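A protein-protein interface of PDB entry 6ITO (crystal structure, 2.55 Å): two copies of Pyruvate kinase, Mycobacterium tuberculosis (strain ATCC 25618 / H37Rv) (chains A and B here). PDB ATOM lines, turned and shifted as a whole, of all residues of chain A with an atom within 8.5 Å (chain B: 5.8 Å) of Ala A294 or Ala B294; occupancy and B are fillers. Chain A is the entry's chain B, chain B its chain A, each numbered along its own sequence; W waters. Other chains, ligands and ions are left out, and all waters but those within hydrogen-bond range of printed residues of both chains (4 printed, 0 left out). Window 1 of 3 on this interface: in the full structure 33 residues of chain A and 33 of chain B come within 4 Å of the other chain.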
ATOM      1  N   ARG A 245      10.238   8.514 -35.417  1.00  0.00           N
ATOM      2  CA  ARG A 245      11.325   9.366 -34.872  1.00  0.00           C
ATOM      3  C   ARG A 245      11.899   8.738 -33.594  1.00  0.00           C
ATOM      4  O   ARG A 245      13.096   8.968 -33.319  1.00  0.00           O
ATOM      5  CB  ARG A 245      10.793  10.782 -34.650  1.00  0.00           C
ATOM      6  CG  ARG A 245      10.285  11.429 -35.929  1.00  0.00           C
ATOM      7  CD  ARG A 245       9.841  12.858 -35.747  1.00  0.00           C
ATOM      8  NE  ARG A 245       9.051  13.044 -34.546  1.00  0.00           N
ATOM      9  CZ  ARG A 245       8.723  14.217 -34.052  1.00  0.00           C
ATOM     10  NH1 ARG A 245       8.041  14.286 -32.930  1.00  0.00           N
ATOM     11  NH2 ARG A 245       9.097  15.322 -34.665  1.00  0.00           N
ATOM     12  N   GLY A 246      11.076   7.987 -32.849  1.00  0.00           N
ATOM     13  CA  GLY A 246      11.498   7.167 -31.702  1.00  0.00           C
ATOM     14  C   GLY A 246      12.734   6.344 -32.022  1.00  0.00           C
ATOM     15  O   GLY A 246      13.790   6.594 -31.400  1.00  0.00           O
ATOM     16  N   LEU A 254      20.323  11.689 -32.654  1.00  0.00           N
ATOM     17  CA  LEU A 254      18.992  12.300 -32.465  1.00  0.00           C
ATOM     18  C   LEU A 254      19.002  13.705 -33.072  1.00  0.00           C
ATOM     19  O   LEU A 254      17.945  14.178 -33.459  1.00  0.00           O
ATOM     20  CB  LEU A 254      18.628  12.308 -30.977  1.00  0.00           C
ATOM     21  CG  LEU A 254      19.465  13.204 -30.069  1.00  0.00           C
ATOM     22  CD1 LEU A 254      19.018  14.648 -30.159  1.00  0.00           C
ATOM     23  CD2 LEU A 254      19.394  12.725 -28.629  1.00  0.00           C
ATOM     24  N   VAL A 257      17.784  13.943 -36.900  1.00  0.00           N
ATOM     25  CA  VAL A 257      16.385  13.532 -37.210  1.00  0.00           C
ATOM     26  C   VAL A 257      15.625  14.715 -37.797  1.00  0.00           C
ATOM     27  O   VAL A 257      14.945  14.564 -38.792  1.00  0.00           O
ATOM     28  CB  VAL A 257      15.669  12.958 -35.980  1.00  0.00           C
ATOM     29  CG1 VAL A 257      14.180  12.782 -36.231  1.00  0.00           C
ATOM     30  CG2 VAL A 257      16.297  11.653 -35.533  1.00  0.00           C
ATOM     31  N   PRO A 258      15.699  15.917 -37.205  1.00  0.00           N
ATOM     32  CA  PRO A 258      14.934  17.050 -37.701  1.00  0.00           C
ATOM     33  C   PRO A 258      15.043  17.279 -39.217  1.00  0.00           C
ATOM     34  O   PRO A 258      14.078  17.624 -39.815  1.00  0.00           O
ATOM     35  CB  PRO A 258      15.551  18.214 -36.919  1.00  0.00           C
ATOM     36  CG  PRO A 258      15.905  17.591 -35.608  1.00  0.00           C
ATOM     37  CD  PRO A 258      16.458  16.244 -35.995  1.00  0.00           C
ATOM     38  N   GLN A 261      13.531  14.181 -41.294  1.00  0.00           N
ATOM     39  CA  GLN A 261      12.075  14.418 -41.312  1.00  0.00           C
ATOM     40  C   GLN A 261      11.755  15.330 -42.495  1.00  0.00           C
ATOM     41  O   GLN A 261      10.901  14.939 -43.360  1.00  0.00           O
ATOM     42  CB  GLN A 261      11.602  15.034 -39.980  1.00  0.00           C
ATOM     43  CG  GLN A 261      10.211  15.647 -40.053  1.00  0.00           C
ATOM     44  CD  GLN A 261       9.678  16.071 -38.713  1.00  0.00           C
ATOM     45  OE1 GLN A 261       9.903  15.414 -37.706  1.00  0.00           O
ATOM     46  NE2 GLN A 261       8.968  17.192 -38.695  1.00  0.00           N
ATOM     47  N   ALA A 278       5.741  10.912 -36.746  1.00  0.00           N
ATOM     48  CA  ALA A 278       5.359  10.055 -35.602  1.00  0.00           C
ATOM     49  C   ALA A 278       6.309  10.233 -34.404  1.00  0.00           C
ATOM     50  O   ALA A 278       7.539  10.412 -34.608  1.00  0.00           O
ATOM     51  CB  ALA A 278       5.317   8.621 -36.039  1.00  0.00           C
ATOM     52  N   THR A 279       5.724  10.211 -33.203  1.00  0.00           N
ATOM     53  CA  THR A 279       6.347   9.798 -31.930  1.00  0.00           C
ATOM     54  C   THR A 279       6.852  11.026 -31.170  1.00  0.00           C
ATOM     55  O   THR A 279       7.729  11.738 -31.706  1.00  0.00           O
ATOM     56  CB  THR A 279       7.440   8.770 -32.177  1.00  0.00           C
ATOM     57  OG1 THR A 279       6.806   7.642 -32.780  1.00  0.00           O
ATOM     58  CG2 THR A 279       8.160   8.373 -30.910  1.00  0.00           C
ATOM     59  N   GLN A 280       6.267  11.261 -29.987  1.00  0.00           N
ATOM     60  CA  GLN A 280       6.699  12.234 -28.936  1.00  0.00           C
ATOM     61  C   GLN A 280       6.352  13.670 -29.342  1.00  0.00           C
ATOM     62  O   GLN A 280       6.855  14.598 -28.703  1.00  0.00           O
ATOM     63  CB  GLN A 280       8.184  12.091 -28.660  1.00  0.00           C
ATOM     64  CG  GLN A 280       8.531  10.776 -28.015  1.00  0.00           C
ATOM     65  CD  GLN A 280       9.847  10.848 -27.314  1.00  0.00           C
ATOM     66  OE1 GLN A 280      10.830  11.329 -27.860  1.00  0.00           O
ATOM     67  NE2 GLN A 280       9.862  10.392 -26.080  1.00  0.00           N
ATOM     68  N   MET A 281       5.469  13.840 -30.301  1.00  0.00           N
ATOM     69  CA  MET A 281       5.031  15.174 -30.746  1.00  0.00           C
ATOM     70  C   MET A 281       4.447  15.926 -29.552  1.00  0.00           C
ATOM     71  O   MET A 281       4.709  17.114 -29.438  1.00  0.00           O
ATOM     72  CB  MET A 281       3.999  15.085 -31.876  1.00  0.00           C
ATOM     73  CG  MET A 281       4.499  14.294 -33.076  1.00  0.00           C
ATOM     74  SD  MET A 281       3.883  14.909 -34.668  1.00  0.00           S
ATOM     75  CE  MET A 281       5.051  16.245 -34.973  1.00  0.00           C
ATOM     76  N   LEU A 282       3.719  15.231 -28.686  1.00  0.00           N
ATOM     77  CA  LEU A 282       3.127  15.810 -27.449  1.00  0.00           C
ATOM     78  C   LEU A 282       3.421  14.870 -26.264  1.00  0.00           C
ATOM     79  O   LEU A 282       2.538  14.700 -25.386  1.00  0.00           O
ATOM     80  CB  LEU A 282       1.620  16.024 -27.666  1.00  0.00           C
ATOM     81  CG  LEU A 282       1.244  17.048 -28.749  1.00  0.00           C
ATOM     82  CD1 LEU A 282      -0.229  16.934 -29.122  1.00  0.00           C
ATOM     83  CD2 LEU A 282       1.582  18.475 -28.309  1.00  0.00           C
ATOM     84  N   ASP A 283       4.639  14.332 -26.209  1.00  0.00           N
ATOM     85  CA  ASP A 283       5.037  13.275 -25.245  1.00  0.00           C
ATOM     86  C   ASP A 283       4.535  13.625 -23.838  1.00  0.00           C
ATOM     87  O   ASP A 283       4.073  12.700 -23.137  1.00  0.00           O
ATOM     88  CB  ASP A 283       6.547  13.049 -25.210  1.00  0.00           C
ATOM     89  CG  ASP A 283       6.918  11.880 -24.316  1.00  0.00           C
ATOM     90  OD1 ASP A 283       6.630  10.751 -24.708  1.00  0.00           O
ATOM     91  OD2 ASP A 283       7.399  12.123 -23.193  1.00  0.00           O
ATOM     92  N   SER A 284       4.679  14.885 -23.413  1.00  0.00           N
ATOM     93  CA  SER A 284       4.467  15.316 -22.003  1.00  0.00           C
ATOM     94  C   SER A 284       2.974  15.226 -21.636  1.00  0.00           C
ATOM     95  O   SER A 284       2.670  15.258 -20.440  1.00  0.00           O
ATOM     96  CB  SER A 284       5.043  16.690 -21.742  1.00  0.00           C
ATOM     97  OG  SER A 284       4.111  17.713 -22.029  1.00  0.00           O
ATOM     98  N   PRO A 291       0.774  20.569 -23.229  1.00  0.00           N
ATOM     99  CA  PRO A 291       2.105  20.164 -23.672  1.00  0.00           C
ATOM    100  C   PRO A 291       3.208  21.194 -23.346  1.00  0.00           C
ATOM    101  O   PRO A 291       2.909  22.230 -22.804  1.00  0.00           O
ATOM    102  CB  PRO A 291       1.891  20.038 -25.186  1.00  0.00           C
ATOM    103  CG  PRO A 291       0.906  21.141 -25.492  1.00  0.00           C
ATOM    104  CD  PRO A 291       0.006  21.224 -24.275  1.00  0.00           C
ATOM    105  N   THR A 292       4.445  20.886 -23.705  1.00  0.00           N
ATOM    106  CA  THR A 292       5.601  21.819 -23.611  1.00  0.00           C
ATOM    107  C   THR A 292       5.574  22.774 -24.811  1.00  0.00           C
ATOM    108  O   THR A 292       4.850  22.501 -25.792  1.00  0.00           O
ATOM    109  CB  THR A 292       6.933  21.063 -23.501  1.00  0.00           C
ATOM    110  OG1 THR A 292       7.187  20.390 -24.733  1.00  0.00           O
ATOM    111  CG2 THR A 292       6.946  20.060 -22.369  1.00  0.00           C
ATOM    112  N   ARG A 293       6.297  23.871 -24.710  1.00  0.00           N
ATOM    113  CA  ARG A 293       6.412  24.863 -25.789  1.00  0.00           C
ATOM    114  C   ARG A 293       7.139  24.211 -26.965  1.00  0.00           C
ATOM    115  O   ARG A 293       6.785  24.504 -28.103  1.00  0.00           O
ATOM    116  CB  ARG A 293       7.128  26.104 -25.271  1.00  0.00           C
ATOM    117  CG  ARG A 293       6.476  26.711 -24.049  1.00  0.00           C
ATOM    118  CD  ARG A 293       5.181  27.386 -24.375  1.00  0.00           C
ATOM    119  NE  ARG A 293       4.549  27.852 -23.170  1.00  0.00           N
ATOM    120  CZ  ARG A 293       3.728  27.129 -22.428  1.00  0.00           C
ATOM    121  NH1 ARG A 293       3.401  25.904 -22.801  1.00  0.00           N
ATOM    122  NH2 ARG A 293       3.218  27.642 -21.326  1.00  0.00           N
ATOM    123  N   ALA A 294       8.082  23.323 -26.679  1.00  0.00           N
ATOM    124  CA  ALA A 294       8.808  22.508 -27.678  1.00  0.00           C
ATOM    125  C   ALA A 294       7.818  21.654 -28.455  1.00  0.00           C
ATOM    126  O   ALA A 294       7.968  21.519 -29.678  1.00  0.00           O
ATOM    127  CB  ALA A 294       9.829  21.640 -26.990  1.00  0.00           C
ATOM    128  N   GLU A 295       6.891  21.035 -27.743  1.00  0.00           N
ATOM    129  CA  GLU A 295       5.904  20.105 -28.316  1.00  0.00           C
ATOM    130  C   GLU A 295       4.965  20.888 -29.231  1.00  0.00           C
ATOM    131  O   GLU A 295       4.903  20.558 -30.406  1.00  0.00           O
ATOM    132  CB  GLU A 295       5.200  19.350 -27.191  1.00  0.00           C
ATOM    133  CG  GLU A 295       6.066  18.242 -26.615  1.00  0.00           C
ATOM    134  CD  GLU A 295       5.667  17.735 -25.256  1.00  0.00           C
ATOM    135  OE1 GLU A 295       4.708  18.280 -24.662  1.00  0.00           O
ATOM    136  OE2 GLU A 295       6.324  16.805 -24.791  1.00  0.00           O
ATOM    137  N   ALA A 296       4.355  21.949 -28.736  1.00  0.00           N
ATOM    138  CA  ALA A 296       3.543  22.865 -29.549  1.00  0.00           C
ATOM    139  C   ALA A 296       4.317  23.221 -30.832  1.00  0.00           C
ATOM    140  O   ALA A 296       3.742  23.074 -31.923  1.00  0.00           O
ATOM    141  CB  ALA A 296       3.172  24.080 -28.754  1.00  0.00           C
ATOM    142  N   SER A 297       5.586  23.628 -30.705  1.00  0.00           N
ATOM    143  CA  SER A 297       6.478  24.010 -31.842  1.00  0.00           C
ATOM    144  C   SER A 297       6.648  22.818 -32.800  1.00  0.00           C
ATOM    145  O   SER A 297       6.622  23.023 -34.044  1.00  0.00           O
ATOM    146  CB  SER A 297       7.837  24.521 -31.340  1.00  0.00           C
ATOM    147  OG  SER A 297       8.723  24.784 -32.429  1.00  0.00           O
ATOM    148  N   ASP A 298       6.864  21.634 -32.256  1.00  0.00           N
ATOM    149  CA  ASP A 298       7.204  20.434 -33.052  1.00  0.00           C
ATOM    150  C   ASP A 298       6.046  20.148 -34.002  1.00  0.00           C
ATOM    151  O   ASP A 298       6.309  19.912 -35.207  1.00  0.00           O
ATOM    152  CB  ASP A 298       7.497  19.232 -32.166  1.00  0.00           C
ATOM    153  CG  ASP A 298       7.785  17.988 -32.966  1.00  0.00           C
ATOM    154  OD1 ASP A 298       8.413  18.108 -34.029  1.00  0.00           O
ATOM    155  OD2 ASP A 298       7.354  16.941 -32.549  1.00  0.00           O
ATOM    156  N   VAL A 299       4.820  20.243 -33.493  1.00  0.00           N
ATOM    157  CA  VAL A 299       3.568  19.981 -34.249  1.00  0.00           C
ATOM    158  C   VAL A 299       3.394  21.065 -35.335  1.00  0.00           C
ATOM    159  O   VAL A 299       3.185  20.701 -36.498  1.00  0.00           O
ATOM    160  CB  VAL A 299       2.361  19.907 -33.292  1.00  0.00           C
ATOM    161  CG1 VAL A 299       1.043  19.877 -34.041  1.00  0.00           C
ATOM    162  CG2 VAL A 299       2.470  18.721 -32.336  1.00  0.00           C
ATOM    163  N   ALA A 300       3.485  22.341 -34.974  1.00  0.00           N
ATOM    164  CA  ALA A 300       3.371  23.493 -35.909  1.00  0.00           C
ATOM    165  C   ALA A 300       4.360  23.319 -37.060  1.00  0.00           C
ATOM    166  O   ALA A 300       3.973  23.560 -38.203  1.00  0.00           O
ATOM    167  CB  ALA A 300       3.618  24.780 -35.183  1.00  0.00           C
ATOM    168  N   ASN A 301       5.573  22.867 -36.763  1.00  0.00           N
ATOM    169  CA  ASN A 301       6.690  22.783 -37.740  1.00  0.00           C
ATOM    170  C   ASN A 301       6.484  21.577 -38.670  1.00  0.00           C
ATOM    171  O   ASN A 301       6.871  21.673 -39.843  1.00  0.00           O
ATOM    172  CB  ASN A 301       8.064  22.755 -37.031  1.00  0.00           C
ATOM    173  CG  ASN A 301       8.606  24.150 -36.759  1.00  0.00           C
ATOM    174  OD1 ASN A 301       8.753  24.944 -37.680  1.00  0.00           O
ATOM    175  ND2 ASN A 301       8.855  24.470 -35.495  1.00  0.00           N
ATOM    176  N   GLU A 315       0.528   9.058 -26.265  1.00  0.00           N
ATOM    177  CA  GLU A 315      -0.394  10.144 -25.869  1.00  0.00           C
ATOM    178  C   GLU A 315      -1.818   9.592 -25.818  1.00  0.00           C
ATOM    179  O   GLU A 315      -2.565  10.030 -24.949  1.00  0.00           O
ATOM    180  CB  GLU A 315      -0.279  11.328 -26.823  1.00  0.00           C
ATOM    181  CG  GLU A 315       1.081  12.005 -26.790  1.00  0.00           C
ATOM    182  CD  GLU A 315       2.020  11.595 -27.905  1.00  0.00           C
ATOM    183  OE1 GLU A 315       2.138  10.393 -28.161  1.00  0.00           O
ATOM    184  OE2 GLU A 315       2.595  12.481 -28.528  1.00  0.00           O
ATOM    185  N   ILE A 332      -3.513  23.198 -32.627  1.00  0.00           N
ATOM    186  CA  ILE A 332      -2.190  23.667 -33.125  1.00  0.00           C
ATOM    187  C   ILE A 332      -2.217  23.650 -34.655  1.00  0.00           C
ATOM    188  O   ILE A 332      -1.878  24.688 -35.276  1.00  0.00           O
ATOM    189  CB  ILE A 332      -1.039  22.827 -32.548  1.00  0.00           C
ATOM    190  CG1 ILE A 332      -0.815  23.125 -31.066  1.00  0.00           C
ATOM    191  CG2 ILE A 332       0.222  23.038 -33.338  1.00  0.00           C
ATOM    192  CD1 ILE A 332      -0.085  22.024 -30.314  1.00  0.00           C
ATOM    193  N   ARG B 245       8.547  31.941 -23.837  1.00  0.00           N
ATOM    194  CA  ARG B 245       7.452  31.088 -24.363  1.00  0.00           C
ATOM    195  C   ARG B 245       6.627  30.494 -23.204  1.00  0.00           C
ATOM    196  O   ARG B 245       5.432  30.225 -23.418  1.00  0.00           O
ATOM    197  CB  ARG B 245       8.042  30.016 -25.273  1.00  0.00           C
ATOM    198  CG  ARG B 245       8.809  30.595 -26.454  1.00  0.00           C
ATOM    199  CD  ARG B 245       9.280  29.542 -27.423  1.00  0.00           C
ATOM    200  NE  ARG B 245       9.872  28.409 -26.741  1.00  0.00           N
ATOM    201  CZ  ARG B 245      10.225  27.289 -27.336  1.00  0.00           C
ATOM    202  NH1 ARG B 245      10.721  26.299 -26.628  1.00  0.00           N
ATOM    203  NH2 ARG B 245      10.074  27.154 -28.638  1.00  0.00           N
ATOM    204  N   THR B 279      12.753  28.799 -23.181  1.00  0.00           N
ATOM    205  CA  THR B 279      11.892  28.094 -22.208  1.00  0.00           C
ATOM    206  C   THR B 279      11.381  26.783 -22.814  1.00  0.00           C
ATOM    207  O   THR B 279      10.660  26.840 -23.840  1.00  0.00           O
ATOM    208  CB  THR B 279      10.755  28.987 -21.731  1.00  0.00           C
ATOM    209  OG1 THR B 279      11.344  30.129 -21.118  1.00  0.00           O
ATOM    210  CG2 THR B 279       9.841  28.282 -20.756  1.00  0.00           C
ATOM    211  N   GLN B 280      11.791  25.660 -22.208  1.00  0.00           N
ATOM    212  CA  GLN B 280      11.277  24.279 -22.434  1.00  0.00           C
ATOM    213  C   GLN B 280      11.794  23.717 -23.760  1.00  0.00           C
ATOM    214  O   GLN B 280      11.273  22.698 -24.202  1.00  0.00           O
ATOM    215  CB  GLN B 280       9.754  24.256 -22.387  1.00  0.00           C
ATOM    216  CG  GLN B 280       9.209  24.579 -21.011  1.00  0.00           C
ATOM    217  CD  GLN B 280       7.810  24.089 -20.851  1.00  0.00           C
ATOM    218  OE1 GLN B 280       6.968  24.286 -21.714  1.00  0.00           O
ATOM    219  NE2 GLN B 280       7.563  23.404 -19.753  1.00  0.00           N
ATOM    220  N   MET B 281      12.834  24.307 -24.315  1.00  0.00           N
ATOM    221  CA  MET B 281      13.440  23.830 -25.570  1.00  0.00           C
ATOM    222  C   MET B 281      13.882  22.384 -25.376  1.00  0.00           C
ATOM    223  O   MET B 281      13.698  21.602 -26.291  1.00  0.00           O
ATOM    224  CB  MET B 281      14.624  24.704 -25.996  1.00  0.00           C
ATOM    225  CG  MET B 281      14.247  26.173 -26.162  1.00  0.00           C
ATOM    226  SD  MET B 281      15.164  27.031 -27.488  1.00  0.00           S
ATOM    227  CE  MET B 281      14.157  26.572 -28.911  1.00  0.00           C
ATOM    228  N   LEU B 282      14.397  22.047 -24.199  1.00  0.00           N
ATOM    229  CA  LEU B 282      14.837  20.670 -23.849  1.00  0.00           C
ATOM    230  C   LEU B 282      14.290  20.311 -22.457  1.00  0.00           C
ATOM    231  O   LEU B 282      15.003  19.639 -21.679  1.00  0.00           O
ATOM    232  CB  LEU B 282      16.376  20.602 -23.915  1.00  0.00           C
ATOM    233  CG  LEU B 282      16.992  20.807 -25.313  1.00  0.00           C
ATOM    234  CD1 LEU B 282      18.486  21.023 -25.231  1.00  0.00           C
ATOM    235  CD2 LEU B 282      16.680  19.629 -26.239  1.00  0.00           C
ATOM    236  N   THR B 292      13.347  14.746 -25.904  1.00  0.00           N
ATOM    237  CA  THR B 292      12.274  14.208 -26.775  1.00  0.00           C
ATOM    238  C   THR B 292      12.566  14.593 -28.227  1.00  0.00           C
ATOM    239  O   THR B 292      13.407  15.475 -28.467  1.00  0.00           O
ATOM    240  CB  THR B 292      10.887  14.670 -26.319  1.00  0.00           C
ATOM    241  OG1 THR B 292      10.772  16.075 -26.547  1.00  0.00           O
ATOM    242  CG2 THR B 292      10.617  14.365 -24.859  1.00  0.00           C
ATOM    243  N   ARG B 293      11.943  13.907 -29.155  1.00  0.00           N
ATOM    244  CA  ARG B 293      12.079  14.176 -30.594  1.00  0.00           C
ATOM    245  C   ARG B 293      11.488  15.556 -30.885  1.00  0.00           C
ATOM    246  O   ARG B 293      12.045  16.257 -31.720  1.00  0.00           O
ATOM    247  CB  ARG B 293      11.404  13.062 -31.383  1.00  0.00           C
ATOM    248  CG  ARG B 293      11.896  11.673 -31.014  1.00  0.00           C
ATOM    249  CD  ARG B 293      13.288  11.423 -31.512  1.00  0.00           C
ATOM    250  NE  ARG B 293      13.754  10.128 -31.092  1.00  0.00           N
ATOM    251  CZ  ARG B 293      14.367   9.887 -29.957  1.00  0.00           C
ATOM    252  NH1 ARG B 293      14.624  10.870 -29.114  1.00  0.00           N
ATOM    253  NH2 ARG B 293      14.743   8.658 -29.670  1.00  0.00           N
ATOM    254  N   ALA B 294      10.442  15.940 -30.165  1.00  0.00           N
ATOM    255  CA  ALA B 294       9.825  17.283 -30.215  1.00  0.00           C
ATOM    256  C   ALA B 294      10.851  18.333 -29.824  1.00  0.00           C
ATOM    257  O   ALA B 294      10.887  19.403 -30.453  1.00  0.00           O
ATOM    258  CB  ALA B 294       8.639  17.339 -29.292  1.00  0.00           C
ATOM    259  N   GLU B 295      11.593  18.068 -28.764  1.00  0.00           N
ATOM    260  CA  GLU B 295      12.578  19.005 -28.198  1.00  0.00           C
ATOM    261  C   GLU B 295      13.717  19.188 -29.196  1.00  0.00           C
ATOM    262  O   GLU B 295      13.936  20.326 -29.616  1.00  0.00           O
ATOM    263  CB  GLU B 295      13.026  18.508 -26.830  1.00  0.00           C
ATOM    264  CG  GLU B 295      11.996  18.786 -25.750  1.00  0.00           C
ATOM    265  CD  GLU B 295      12.134  17.970 -24.493  1.00  0.00           C
ATOM    266  OE1 GLU B 295      13.024  17.095 -24.435  1.00  0.00           O
ATOM    267  OE2 GLU B 295      11.339  18.205 -23.581  1.00  0.00           O
ATOM    268  N   ALA B 296      14.330  18.105 -29.649  1.00  0.00           N
ATOM    269  CA  ALA B 296      15.333  18.143 -30.726  1.00  0.00           C
ATOM    270  C   ALA B 296      14.795  19.009 -31.884  1.00  0.00           C
ATOM    271  O   ALA B 296      15.522  19.921 -32.321  1.00  0.00           O
ATOM    272  CB  ALA B 296      15.673  16.756 -31.165  1.00  0.00           C
ATOM    273  N   SER B 297      13.554  18.764 -32.333  1.00  0.00           N
ATOM    274  CA  SER B 297      12.890  19.502 -33.455  1.00  0.00           C
ATOM    275  C   SER B 297      12.786  20.993 -33.105  1.00  0.00           C
ATOM    276  O   SER B 297      13.032  21.849 -33.993  1.00  0.00           O
ATOM    277  CB  SER B 297      11.503  18.899 -33.784  1.00  0.00           C
ATOM    278  OG  SER B 297      10.798  19.687 -34.740  1.00  0.00           O
ATOM    279  N   ASP B 298      12.395  21.295 -31.882  1.00  0.00           N
ATOM    280  CA  ASP B 298      12.086  22.676 -31.459  1.00  0.00           C
ATOM    281  C   ASP B 298      13.353  23.515 -31.605  1.00  0.00           C
ATOM    282  O   ASP B 298      13.265  24.631 -32.168  1.00  0.00           O
ATOM    283  CB  ASP B 298      11.555  22.718 -30.036  1.00  0.00           C
ATOM    284  CG  ASP B 298      11.307  24.121 -29.560  1.00  0.00           C
ATOM    285  OD1 ASP B 298      10.862  24.953 -30.383  1.00  0.00           O
ATOM    286  OD2 ASP B 298      11.585  24.380 -28.410  1.00  0.00           O
ATOM    287  N   VAL B 299      14.487  22.961 -31.173  1.00  0.00           N
ATOM    288  CA  VAL B 299      15.819  23.617 -31.209  1.00  0.00           C
ATOM    289  C   VAL B 299      16.254  23.809 -32.678  1.00  0.00           C
ATOM    290  O   VAL B 299      16.613  24.937 -33.039  1.00  0.00           O
ATOM    291  CB  VAL B 299      16.842  22.800 -30.398  1.00  0.00           C
ATOM    292  CG1 VAL B 299      18.262  23.292 -30.610  1.00  0.00           C
ATOM    293  CG2 VAL B 299      16.492  22.778 -28.912  1.00  0.00           C
HETATM  294  O   HOH W   1      12.114  18.327 -37.010  1.00  0.00           O
HETATM  295  O   HOH W   2       8.324  18.624 -36.709  1.00  0.00           O
HETATM  296  O   HOH W   3      11.286  26.643 -32.327  1.00  0.00           O
HETATM  297  O   HOH W   4       8.776  17.058 -23.076  1.00  0.00           O
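The guanidinium group of Arg B245 sits at hydrogen-bond distance from the backbone carbonyl oxygen of Thr B279 (2.8 Å). The side-chain carboxylate (OD2) of Asp B298 is in salt-bridge range of the guanidinium group (NH1) of Arg B245 (2.8 Å). The backbone NH (N) of Thr B292 lies within hydrogen-bond range of the side-chain carboxylate (OE1) of Glu B295, 2.8 Å away. O of Thr A279 is in hydrogen-bond range of NH1 of Arg A245, at 2.8 Å. The backbone carbonyl oxygen (O) of Ser A297 lies within hydrogen-bond range of the side-chain amide nitrogen (ND2) of Asn A301 (3.0 Å).
Of chain B, only Arg B245 (3.98 Å), Gln B280 (3.3 Å), Met B281 (3.9 Å), Ala B294 (3.7 Å), Glu B295 (3.8 Å) and Asp B298 (3.4 Å) come within 4 Å of Ala A294. Of the printed residues of chain A, Ala B294 touches Gln A280, Met A281, Ala A294, Glu A295 and Asp A298. Printed residues of chain B within 4 Å of Arg A293: Arg B245, Thr B279 and Gln B280. Printed residues of chain A within 4 Å of Asp B298: Ala A294 and Ser A297. Of the printed residues of chain A, Ser B297 touches Asp A298. Of the printed residues of chain B, Asp A298 touches Ala B294 (3.4 Å) and Ser B297 (2.9 Å). Of the printed residues of chain B, Glu A295 touches Ala B294. Val A299 touches none of the printed residues of chain B. Ile A332 touches none of the printed residues of chain B. The nearest residue of chain B that does not touch Ala A294 is Thr B279 (5.2 Å).
Water W2 lies within hydrogen-bond range of the side-chain amide nitrogen of Gln A261 (2.5 Å), the side-chain carboxylate of Asp A298 (2.7 Å) and the side-chain hydroxyl of Ser B297 (3.3 Å). Water W3 bridges the side-chain carboxylate (OD1) of Asp B298 (2.6 Å) and the side-chain hydroxyl (OG) of Ser A297 (3.2 Å). Water W4 lies within hydrogen-bond range of the side-chain carboxylate of Glu B295 (2.9 Å) and the side-chain carboxylate of Glu A295 (3.0 Å). Water W1 lies within hydrogen-bond range of the side-chain hydroxyl (OG) of Ser B297 (3.0 Å) and the backbone carbonyl oxygen (O) of Pro A258 (3.5 Å).
The backbone carbonyl oxygen (O) of Arg B245 is in hydrogen-bond range of the guanidinium group (NE) of Arg A293 (2.5 Å). The side-chain amide oxygen of Gln B280 sits at hydrogen-bond distance from the backbone NH of Arg A293. The guanidinium group of Arg B293 is in hydrogen-bond range of the backbone carbonyl oxygen of Arg A245 (2.6 Å). O of Gly A246 sits at hydrogen-bond distance from NH2 of Arg B293. The backbone NH (N) of Arg B293 is in hydrogen-bond range of the side-chain amide oxygen (OE1) of Gln A280 (3.1 Å). The side-chain hydroxyl (OG) of Ser B297 lies within hydrogen-bond range of the side-chain carboxylate (OD1) of Asp A298. The side-chain carboxylate (OD1) of Asp B298 lies within hydrogen-bond range of the side-chain hydroxyl (OG) of Ser A297 (3.0 Å).
Among the printed residues, 21 pairs touch across the chains. Among the printed residues, no Asp or Glu carboxylate lies within 4 Å of a Lys or Arg side-chain nitrogen of the other chain.
Among the printed residues, merely in contact across the chains: Thr A279 with Arg B293 (3.9 Å), Gln A280 with Thr B292 (3.4 Å), Gln A280 with Ala B294 (3.3 Å), Met A281 with Ala B294 (3.9 Å), Thr A292 with Gln B280 (3.4 Å), Arg A293 with Thr B279 (3.9 Å), Ala A294 with Arg B245 (3.98 Å), Ala A294 with Gln B280 (3.3 Å), Ala A294 with Met B281 (3.9 Å), Ala A294 with Ala B294 (3.7 Å), Ala A294 with Glu B295 (3.8 Å), Ala A294 with Asp B298 (3.4 Å), Glu A295 with Ala B294 (3.8 Å) and Asp A298 with Ala B294 (3.4 Å).
Gln A280 touches Arg B293, and with the chains exchanged Arg A293 touches Gln B280. Gln A280 touches Ala B294, and with the chains exchanged Ala A294 touches Gln B280. Ala A294 touches Arg B245, but with the chains exchanged Arg A245 does not touch Ala B294 (4.02 Å). Ala B294 touches its own counterpart, Ala A294.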
